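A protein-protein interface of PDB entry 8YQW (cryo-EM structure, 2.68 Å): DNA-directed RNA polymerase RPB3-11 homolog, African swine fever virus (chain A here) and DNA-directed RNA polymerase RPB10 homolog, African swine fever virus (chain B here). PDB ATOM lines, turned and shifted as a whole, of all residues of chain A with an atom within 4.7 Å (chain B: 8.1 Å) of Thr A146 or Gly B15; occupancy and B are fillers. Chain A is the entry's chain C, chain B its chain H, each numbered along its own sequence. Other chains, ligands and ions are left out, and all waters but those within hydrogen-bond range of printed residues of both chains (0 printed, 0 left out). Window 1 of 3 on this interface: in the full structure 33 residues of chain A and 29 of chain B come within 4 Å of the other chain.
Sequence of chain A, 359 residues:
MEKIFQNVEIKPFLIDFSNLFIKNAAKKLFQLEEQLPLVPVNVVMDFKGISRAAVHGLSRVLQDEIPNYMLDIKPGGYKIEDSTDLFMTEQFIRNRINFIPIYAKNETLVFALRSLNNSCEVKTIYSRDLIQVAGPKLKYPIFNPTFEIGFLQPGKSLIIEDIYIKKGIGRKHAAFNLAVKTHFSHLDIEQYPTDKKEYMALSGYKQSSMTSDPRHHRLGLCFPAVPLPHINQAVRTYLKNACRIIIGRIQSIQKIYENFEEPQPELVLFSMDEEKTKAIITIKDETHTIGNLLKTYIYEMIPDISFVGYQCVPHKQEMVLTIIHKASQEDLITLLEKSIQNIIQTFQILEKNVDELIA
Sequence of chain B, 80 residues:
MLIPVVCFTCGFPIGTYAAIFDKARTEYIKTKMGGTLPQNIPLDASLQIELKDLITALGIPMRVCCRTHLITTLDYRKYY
Ala B19 touches Phe A30 (CB to CZ, 3.7 Å). Phe A30 touches Ile B20 (CE2 to CG1, 3.6 Å). Thr B16 touches Leu A36. Thr B16 touches Asn A144. Gly B15 touches Thr A146. Val B5 touches Phe A147 (CG1 to CE1, 3.6 Å). CD1 of Phe A147 touches C of Gly B15, 3.9 Å away. Thr B16 touches Phe A147. CB of Ala B19 touches OE2 of Glu A148, at 3.5 Å.
Printed residues of chain B within 4 Å of Leu A36: Thr B16 (3.4 Å). Of the printed residues of chain B, Asn A144 touches Thr B16 (3.5 Å). No residue of chain B comes within 4 Å of Pro A145. Thr A146 touches just these residues of chain B: Gly B15 and Thr B16. Printed residues of chain B within 4 Å of Glu A148: Ala B19 (3.5 Å). Gly B11 touches none of the printed residues of chain A. Of the printed residues of chain A, Gly B15 touches Thr A146 (3.6 Å) and Phe A147 (3.9 Å). Of the printed residues of chain A, Ala B19 touches Phe A30 (3.7 Å) and Glu A148 (3.5 Å). Printed residues of chain A within 4 Å of Ile B20: Phe A30 (3.6 Å). Ile B60 touches none of the printed residues of chain A. The nearest residue of chain B that does not touch Thr A146 is Ala B19 (4.6 Å).
OG1 of Thr A146 lies within hydrogen-bond range of OG1 of Thr B16.
Hydrophobic or aromatic side chains of chain A within 4 Å of the printed part of chain B: Phe A30, Leu A36 and Phe A147. Of the 18 printed residues of chain B, 5 touch a printed residue of chain A. Hydrophobic or aromatic side chains of chain B within 4 Å of the printed part of chain A: Val B5, Ala B19 and Ile B20. Among the printed residues, no Asp or Glu carboxylate lies within 4 Å of a Lys or Arg side-chain nitrogen of the other chain.
The side-chain hydroxyl (OG) of Ser A127 sits at hydrogen-bond distance from the backbone carbonyl oxygen (O) of Asn A144 (2.6 Å). The side-chain hydroxyl (OG) of Ser A127 lies within hydrogen-bond range of the backbone NH (N) of Thr A146 (3.4 Å). N of Ser A127 sits at hydrogen-bond distance from O of Phe A147 (2.8 Å). O of Pro B4 is in hydrogen-bond range of N of Gly B15, 3.5 Å away. The backbone NH of Ile B14 sits at hydrogen-bond distance from the backbone carbonyl oxygen of Val B5, at 3.3 Å. The backbone carbonyl oxygen (O) of Val B5 lies within hydrogen-bond range of the backbone NH (N) of Gly B15, at 2.6 Å.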
ATOM      1  N   PHE A  30     -17.797 -11.744   2.862  1.00  0.00           N
ATOM      2  CA  PHE A  30     -19.213 -11.664   3.193  1.00  0.00           C
ATOM      3  C   PHE A  30     -19.980 -12.937   2.859  1.00  0.00           C
ATOM      4  O   PHE A  30     -21.209 -12.952   2.987  1.00  0.00           O
ATOM      5  CB  PHE A  30     -19.852 -10.476   2.470  1.00  0.00           C
ATOM      6  CG  PHE A  30     -19.097  -9.190   2.635  1.00  0.00           C
ATOM      7  CD1 PHE A  30     -19.187  -8.464   3.809  1.00  0.00           C
ATOM      8  CD2 PHE A  30     -18.298  -8.706   1.615  1.00  0.00           C
ATOM      9  CE1 PHE A  30     -18.494  -7.285   3.960  1.00  0.00           C
ATOM     10  CE2 PHE A  30     -17.603  -7.526   1.763  1.00  0.00           C
ATOM     11  CZ  PHE A  30     -17.702  -6.816   2.936  1.00  0.00           C
ATOM     12  N   LEU A  36     -25.595  -7.965  -4.963  1.00  0.00           N
ATOM     13  CA  LEU A  36     -26.051  -7.315  -3.748  1.00  0.00           C
ATOM     14  C   LEU A  36     -27.515  -6.899  -3.889  1.00  0.00           C
ATOM     15  O   LEU A  36     -28.012  -6.722  -5.002  1.00  0.00           O
ATOM     16  CB  LEU A  36     -25.176  -6.102  -3.445  1.00  0.00           C
ATOM     17  CG  LEU A  36     -23.759  -6.408  -2.961  1.00  0.00           C
ATOM     18  CD1 LEU A  36     -22.896  -5.160  -3.006  1.00  0.00           C
ATOM     19  CD2 LEU A  36     -23.790  -6.988  -1.562  1.00  0.00           C
ATOM     20  N   SER A 127     -21.857  -2.653   7.635  1.00  0.00           N
ATOM     21  CA  SER A 127     -23.248  -2.222   7.663  1.00  0.00           C
ATOM     22  C   SER A 127     -24.217  -3.380   7.839  1.00  0.00           C
ATOM     23  O   SER A 127     -25.410  -3.138   8.049  1.00  0.00           O
ATOM     24  CB  SER A 127     -23.585  -1.447   6.391  1.00  0.00           C
ATOM     25  OG  SER A 127     -23.439  -2.262   5.246  1.00  0.00           O
ATOM     26  N   ASN A 144     -27.041  -1.814   1.424  1.00  0.00           N
ATOM     27  CA  ASN A 144     -26.171  -2.959   1.226  1.00  0.00           C
ATOM     28  C   ASN A 144     -25.451  -3.318   2.526  1.00  0.00           C
ATOM     29  O   ASN A 144     -25.190  -2.450   3.361  1.00  0.00           O
ATOM     30  CB  ASN A 144     -25.149  -2.669   0.134  1.00  0.00           C
ATOM     31  CG  ASN A 144     -25.745  -2.739  -1.250  1.00  0.00           C
ATOM     32  OD1 ASN A 144     -26.547  -3.621  -1.546  1.00  0.00           O
ATOM     33  ND2 ASN A 144     -25.356  -1.811  -2.110  1.00  0.00           N
ATOM     34  N   PRO A 145     -25.124  -4.594   2.721  1.00  0.00           N
ATOM     35  CA  PRO A 145     -24.407  -5.018   3.932  1.00  0.00           C
ATOM     36  C   PRO A 145     -22.887  -4.996   3.830  1.00  0.00           C
ATOM     37  O   PRO A 145     -22.228  -5.567   4.703  1.00  0.00           O
ATOM     38  CB  PRO A 145     -24.904  -6.457   4.104  1.00  0.00           C
ATOM     39  CG  PRO A 145     -25.081  -6.933   2.713  1.00  0.00           C
ATOM     40  CD  PRO A 145     -25.547  -5.747   1.907  1.00  0.00           C
ATOM     41  N   THR A 146     -22.312  -4.366   2.809  1.00  0.00           N
ATOM     42  CA  THR A 146     -20.881  -4.446   2.554  1.00  0.00           C
ATOM     43  C   THR A 146     -20.144  -3.144   2.841  1.00  0.00           C
ATOM     44  O   THR A 146     -19.014  -2.970   2.374  1.00  0.00           O
ATOM     45  CB  THR A 146     -20.630  -4.874   1.108  1.00  0.00           C
ATOM     46  OG1 THR A 146     -21.372  -4.029   0.223  1.00  0.00           O
ATOM     47  CG2 THR A 146     -21.060  -6.312   0.896  1.00  0.00           C
ATOM     48  N   PHE A 147     -20.744  -2.229   3.594  1.00  0.00           N
ATOM     49  CA  PHE A 147     -20.095  -0.963   3.898  1.00  0.00           C
ATOM     50  C   PHE A 147     -19.233  -1.085   5.144  1.00  0.00           C
ATOM     51  O   PHE A 147     -19.665  -1.629   6.161  1.00  0.00           O
ATOM     52  CB  PHE A 147     -21.133   0.139   4.102  1.00  0.00           C
ATOM     53  CG  PHE A 147     -21.768   0.615   2.836  1.00  0.00           C
ATOM     54  CD1 PHE A 147     -21.188   1.626   2.094  1.00  0.00           C
ATOM     55  CD2 PHE A 147     -22.949   0.055   2.390  1.00  0.00           C
ATOM     56  CE1 PHE A 147     -21.773   2.067   0.929  1.00  0.00           C
ATOM     57  CE2 PHE A 147     -23.537   0.491   1.229  1.00  0.00           C
ATOM     58  CZ  PHE A 147     -22.949   1.501   0.497  1.00  0.00           C
ATOM     59  N   GLU A 148     -18.012  -0.562   5.066  1.00  0.00           N
ATOM     60  CA  GLU A 148     -17.105  -0.523   6.211  1.00  0.00           C
ATOM     61  C   GLU A 148     -17.485   0.679   7.063  1.00  0.00           C
ATOM     62  O   GLU A 148     -17.051   1.802   6.799  1.00  0.00           O
ATOM     63  CB  GLU A 148     -15.654  -0.432   5.754  1.00  0.00           C
ATOM     64  CG  GLU A 148     -15.079  -1.710   5.190  1.00  0.00           C
ATOM     65  CD  GLU A 148     -13.714  -1.494   4.571  1.00  0.00           C
ATOM     66  OE1 GLU A 148     -13.423  -0.351   4.165  1.00  0.00           O
ATOM     67  OE2 GLU A 148     -12.932  -2.463   4.491  1.00  0.00           O
ATOM     68  N   ILE B   3     -11.407   3.716   3.157  1.00  0.00           N
ATOM     69  CA  ILE B   3     -11.907   4.125   1.841  1.00  0.00           C
ATOM     70  C   ILE B   3     -13.289   4.737   2.017  1.00  0.00           C
ATOM     71  O   ILE B   3     -14.155   4.127   2.672  1.00  0.00           O
ATOM     72  CB  ILE B   3     -11.949   2.926   0.879  1.00  0.00           C
ATOM     73  CG1 ILE B   3     -10.533   2.543   0.445  1.00  0.00           C
ATOM     74  CG2 ILE B   3     -12.798   3.237  -0.336  1.00  0.00           C
ATOM     75  CD1 ILE B   3     -10.456   1.229  -0.291  1.00  0.00           C
ATOM     76  N   PRO B   4     -13.553   5.925   1.475  1.00  0.00           N
ATOM     77  CA  PRO B   4     -14.804   6.619   1.794  1.00  0.00           C
ATOM     78  C   PRO B   4     -16.029   5.839   1.342  1.00  0.00           C
ATOM     79  O   PRO B   4     -15.976   5.030   0.415  1.00  0.00           O
ATOM     80  CB  PRO B   4     -14.674   7.944   1.036  1.00  0.00           C
ATOM     81  CG  PRO B   4     -13.706   7.657  -0.055  1.00  0.00           C
ATOM     82  CD  PRO B   4     -12.730   6.690   0.526  1.00  0.00           C
ATOM     83  N   VAL B   5     -17.141   6.081   2.039  1.00  0.00           N
ATOM     84  CA  VAL B   5     -18.394   5.408   1.712  1.00  0.00           C
ATOM     85  C   VAL B   5     -18.837   5.771   0.302  1.00  0.00           C
ATOM     86  O   VAL B   5     -19.307   4.918  -0.459  1.00  0.00           O
ATOM     87  CB  VAL B   5     -19.469   5.761   2.757  1.00  0.00           C
ATOM     88  CG1 VAL B   5     -20.811   5.200   2.347  1.00  0.00           C
ATOM     89  CG2 VAL B   5     -19.072   5.237   4.111  1.00  0.00           C
ATOM     90  N   VAL B   6     -18.693   7.042  -0.068  1.00  0.00           N
ATOM     91  CA  VAL B   6     -19.001   7.513  -1.408  1.00  0.00           C
ATOM     92  C   VAL B   6     -17.786   8.257  -1.942  1.00  0.00           C
ATOM     93  O   VAL B   6     -16.905   8.675  -1.191  1.00  0.00           O
ATOM     94  CB  VAL B   6     -20.249   8.421  -1.441  1.00  0.00           C
ATOM     95  CG1 VAL B   6     -21.481   7.641  -1.035  1.00  0.00           C
ATOM     96  CG2 VAL B   6     -20.051   9.622  -0.541  1.00  0.00           C
ATOM     97  N   CYS B   7     -17.741   8.402  -3.262  1.00  0.00           N
ATOM     98  CA  CYS B   7     -16.686   9.183  -3.888  1.00  0.00           C
ATOM     99  C   CYS B   7     -16.751  10.625  -3.405  1.00  0.00           C
ATOM    100  O   CYS B   7     -17.822  11.235  -3.383  1.00  0.00           O
ATOM    101  CB  CYS B   7     -16.822   9.113  -5.408  1.00  0.00           C
ATOM    102  SG  CYS B   7     -15.742  10.210  -6.328  1.00  0.00           S
ATOM    103  N   GLY B  11     -19.969  11.328  -5.470  1.00  0.00           N
ATOM    104  CA  GLY B  11     -20.882  10.653  -4.575  1.00  0.00           C
ATOM    105  C   GLY B  11     -21.343   9.284  -5.015  1.00  0.00           C
ATOM    106  O   GLY B  11     -22.348   8.793  -4.492  1.00  0.00           O
ATOM    107  N   PHE B  12     -20.657   8.656  -5.964  1.00  0.00           N
ATOM    108  CA  PHE B  12     -20.973   7.280  -6.313  1.00  0.00           C
ATOM    109  C   PHE B  12     -20.627   6.361  -5.143  1.00  0.00           C
ATOM    110  O   PHE B  12     -19.588   6.539  -4.502  1.00  0.00           O
ATOM    111  CB  PHE B  12     -20.206   6.853  -7.564  1.00  0.00           C
ATOM    112  CG  PHE B  12     -20.555   5.477  -8.050  1.00  0.00           C
ATOM    113  CD1 PHE B  12     -21.708   5.258  -8.782  1.00  0.00           C
ATOM    114  CD2 PHE B  12     -19.732   4.400  -7.771  1.00  0.00           C
ATOM    115  CE1 PHE B  12     -22.032   3.995  -9.224  1.00  0.00           C
ATOM    116  CE2 PHE B  12     -20.054   3.136  -8.208  1.00  0.00           C
ATOM    117  CZ  PHE B  12     -21.203   2.934  -8.935  1.00  0.00           C
ATOM    118  N   PRO B  13     -21.474   5.372  -4.838  1.00  0.00           N
ATOM    119  CA  PRO B  13     -21.229   4.525  -3.662  1.00  0.00           C
ATOM    120  C   PRO B  13     -20.022   3.618  -3.817  1.00  0.00           C
ATOM    121  O   PRO B  13     -20.155   2.418  -4.075  1.00  0.00           O
ATOM    122  CB  PRO B  13     -22.525   3.717  -3.538  1.00  0.00           C
ATOM    123  CG  PRO B  13     -23.115   3.733  -4.896  1.00  0.00           C
ATOM    124  CD  PRO B  13     -22.756   5.056  -5.486  1.00  0.00           C
ATOM    125  N   ILE B  14     -18.830   4.197  -3.669  1.00  0.00           N
ATOM    126  CA  ILE B  14     -17.589   3.433  -3.732  1.00  0.00           C
ATOM    127  C   ILE B  14     -17.470   2.463  -2.565  1.00  0.00           C
ATOM    128  O   ILE B  14     -16.934   1.360  -2.721  1.00  0.00           O
ATOM    129  CB  ILE B  14     -16.394   4.402  -3.796  1.00  0.00           C
ATOM    130  CG1 ILE B  14     -16.471   5.234  -5.069  1.00  0.00           C
ATOM    131  CG2 ILE B  14     -15.092   3.667  -3.734  1.00  0.00           C
ATOM    132  CD1 ILE B  14     -16.428   4.392  -6.308  1.00  0.00           C
ATOM    133  N   GLY B  15     -17.970   2.843  -1.388  1.00  0.00           N
ATOM    134  CA  GLY B  15     -17.709   2.071  -0.186  1.00  0.00           C
ATOM    135  C   GLY B  15     -18.242   0.654  -0.221  1.00  0.00           C
ATOM    136  O   GLY B  15     -17.641  -0.247   0.371  1.00  0.00           O
ATOM    137  N   THR B  16     -19.363   0.429  -0.909  1.00  0.00           N
ATOM    138  CA  THR B  16     -19.974  -0.896  -0.898  1.00  0.00           C
ATOM    139  C   THR B  16     -19.101  -1.951  -1.562  1.00  0.00           C
ATOM    140  O   THR B  16     -19.346  -3.146  -1.372  1.00  0.00           O
ATOM    141  CB  THR B  16     -21.343  -0.861  -1.573  1.00  0.00           C
ATOM    142  OG1 THR B  16     -21.873  -2.190  -1.647  1.00  0.00           O
ATOM    143  CG2 THR B  16     -21.237  -0.296  -2.962  1.00  0.00           C
ATOM    144  N   TYR B  17     -18.097  -1.544  -2.335  1.00  0.00           N
ATOM    145  CA  TYR B  17     -17.136  -2.464  -2.922  1.00  0.00           C
ATOM    146  C   TYR B  17     -15.742  -2.292  -2.341  1.00  0.00           C
ATOM    147  O   TYR B  17     -14.800  -2.927  -2.823  1.00  0.00           O
ATOM    148  CB  TYR B  17     -17.089  -2.288  -4.440  1.00  0.00           C
ATOM    149  CG  TYR B  17     -18.448  -2.148  -5.074  1.00  0.00           C
ATOM    150  CD1 TYR B  17     -19.335  -3.211  -5.091  1.00  0.00           C
ATOM    151  CD2 TYR B  17     -18.847  -0.951  -5.648  1.00  0.00           C
ATOM    152  CE1 TYR B  17     -20.577  -3.092  -5.664  1.00  0.00           C
ATOM    153  CE2 TYR B  17     -20.092  -0.821  -6.224  1.00  0.00           C
ATOM    154  CZ  TYR B  17     -20.953  -1.896  -6.227  1.00  0.00           C
ATOM    155  OH  TYR B  17     -22.196  -1.776  -6.800  1.00  0.00           O
ATOM    156  N   ALA B  18     -15.588  -1.448  -1.321  1.00  0.00           N
ATOM    157  CA  ALA B  18     -14.259  -1.142  -0.803  1.00  0.00           C
ATOM    158  C   ALA B  18     -13.605  -2.376  -0.197  1.00  0.00           C
ATOM    159  O   ALA B  18     -12.516  -2.785  -0.619  1.00  0.00           O
ATOM    160  CB  ALA B  18     -14.348  -0.019   0.229  1.00  0.00           C
ATOM    161  N   ALA B  19     -14.273  -2.998   0.778  1.00  0.00           N
ATOM    162  CA  ALA B  19     -13.693  -4.133   1.488  1.00  0.00           C
ATOM    163  C   ALA B  19     -13.228  -5.208   0.519  1.00  0.00           C
ATOM    164  O   ALA B  19     -12.070  -5.640   0.561  1.00  0.00           O
ATOM    165  CB  ALA B  19     -14.709  -4.703   2.476  1.00  0.00           C
ATOM    166  N   ILE B  20     -14.109  -5.614  -0.398  1.00  0.00           N
ATOM    167  CA  ILE B  20     -13.735  -6.601  -1.406  1.00  0.00           C
ATOM    168  C   ILE B  20     -12.523  -6.115  -2.187  1.00  0.00           C
ATOM    169  O   ILE B  20     -11.500  -6.808  -2.274  1.00  0.00           O
ATOM    170  CB  ILE B  20     -14.926  -6.892  -2.335  1.00  0.00           C
ATOM    171  CG1 ILE B  20     -16.137  -7.347  -1.523  1.00  0.00           C
ATOM    172  CG2 ILE B  20     -14.556  -7.934  -3.370  1.00  0.00           C
ATOM    173  CD1 ILE B  20     -17.426  -7.338  -2.303  1.00  0.00           C
ATOM    174  N   PHE B  21     -12.588  -4.879  -2.694  1.00  0.00           N
ATOM    175  CA  PHE B  21     -11.471  -4.349  -3.468  1.00  0.00           C
ATOM    176  C   PHE B  21     -10.188  -4.354  -2.658  1.00  0.00           C
ATOM    177  O   PHE B  21      -9.100  -4.476  -3.229  1.00  0.00           O
ATOM    178  CB  PHE B  21     -11.763  -2.934  -3.959  1.00  0.00           C
ATOM    179  CG  PHE B  21     -10.577  -2.270  -4.594  1.00  0.00           C
ATOM    180  CD1 PHE B  21     -10.166  -2.630  -5.864  1.00  0.00           C
ATOM    181  CD2 PHE B  21      -9.855  -1.307  -3.912  1.00  0.00           C
ATOM    182  CE1 PHE B  21      -9.071  -2.034  -6.443  1.00  0.00           C
ATOM    183  CE2 PHE B  21      -8.760  -0.710  -4.490  1.00  0.00           C
ATOM    184  CZ  PHE B  21      -8.369  -1.072  -5.757  1.00  0.00           C
ATOM    185  N   ILE B  60     -17.744  -0.866 -10.758  1.00  0.00           N
ATOM    186  CA  ILE B  60     -17.481   0.571 -10.629  1.00  0.00           C
ATOM    187  C   ILE B  60     -17.250   1.160 -12.016  1.00  0.00           C
ATOM    188  O   ILE B  60     -16.497   0.575 -12.815  1.00  0.00           O
ATOM    189  CB  ILE B  60     -16.277   0.809  -9.715  1.00  0.00           C
ATOM    190  CG1 ILE B  60     -16.650   0.505  -8.266  1.00  0.00           C
ATOM    191  CG2 ILE B  60     -15.775   2.234  -9.832  1.00  0.00           C
ATOM    192  CD1 ILE B  60     -15.468   0.393  -7.346  1.00  0.00           C
ATOM    193  N   LEU B  70     -10.780   5.380  -4.770  1.00  0.00           N
ATOM    194  CA  LEU B  70     -10.709   3.983  -4.361  1.00  0.00           C
ATOM    195  C   LEU B  70      -9.269   3.495  -4.299  1.00  0.00           C
ATOM    196  O   LEU B  70      -8.878   2.813  -3.345  1.00  0.00           O
ATOM    197  CB  LEU B  70     -11.532   3.127  -5.320  1.00  0.00           C
ATOM    198  CG  LEU B  70     -11.591   1.622  -5.090  1.00  0.00           C
ATOM    199  CD1 LEU B  70     -12.577   1.264  -4.006  1.00  0.00           C
ATOM    200  CD2 LEU B  70     -11.961   0.942  -6.386  1.00  0.00           C
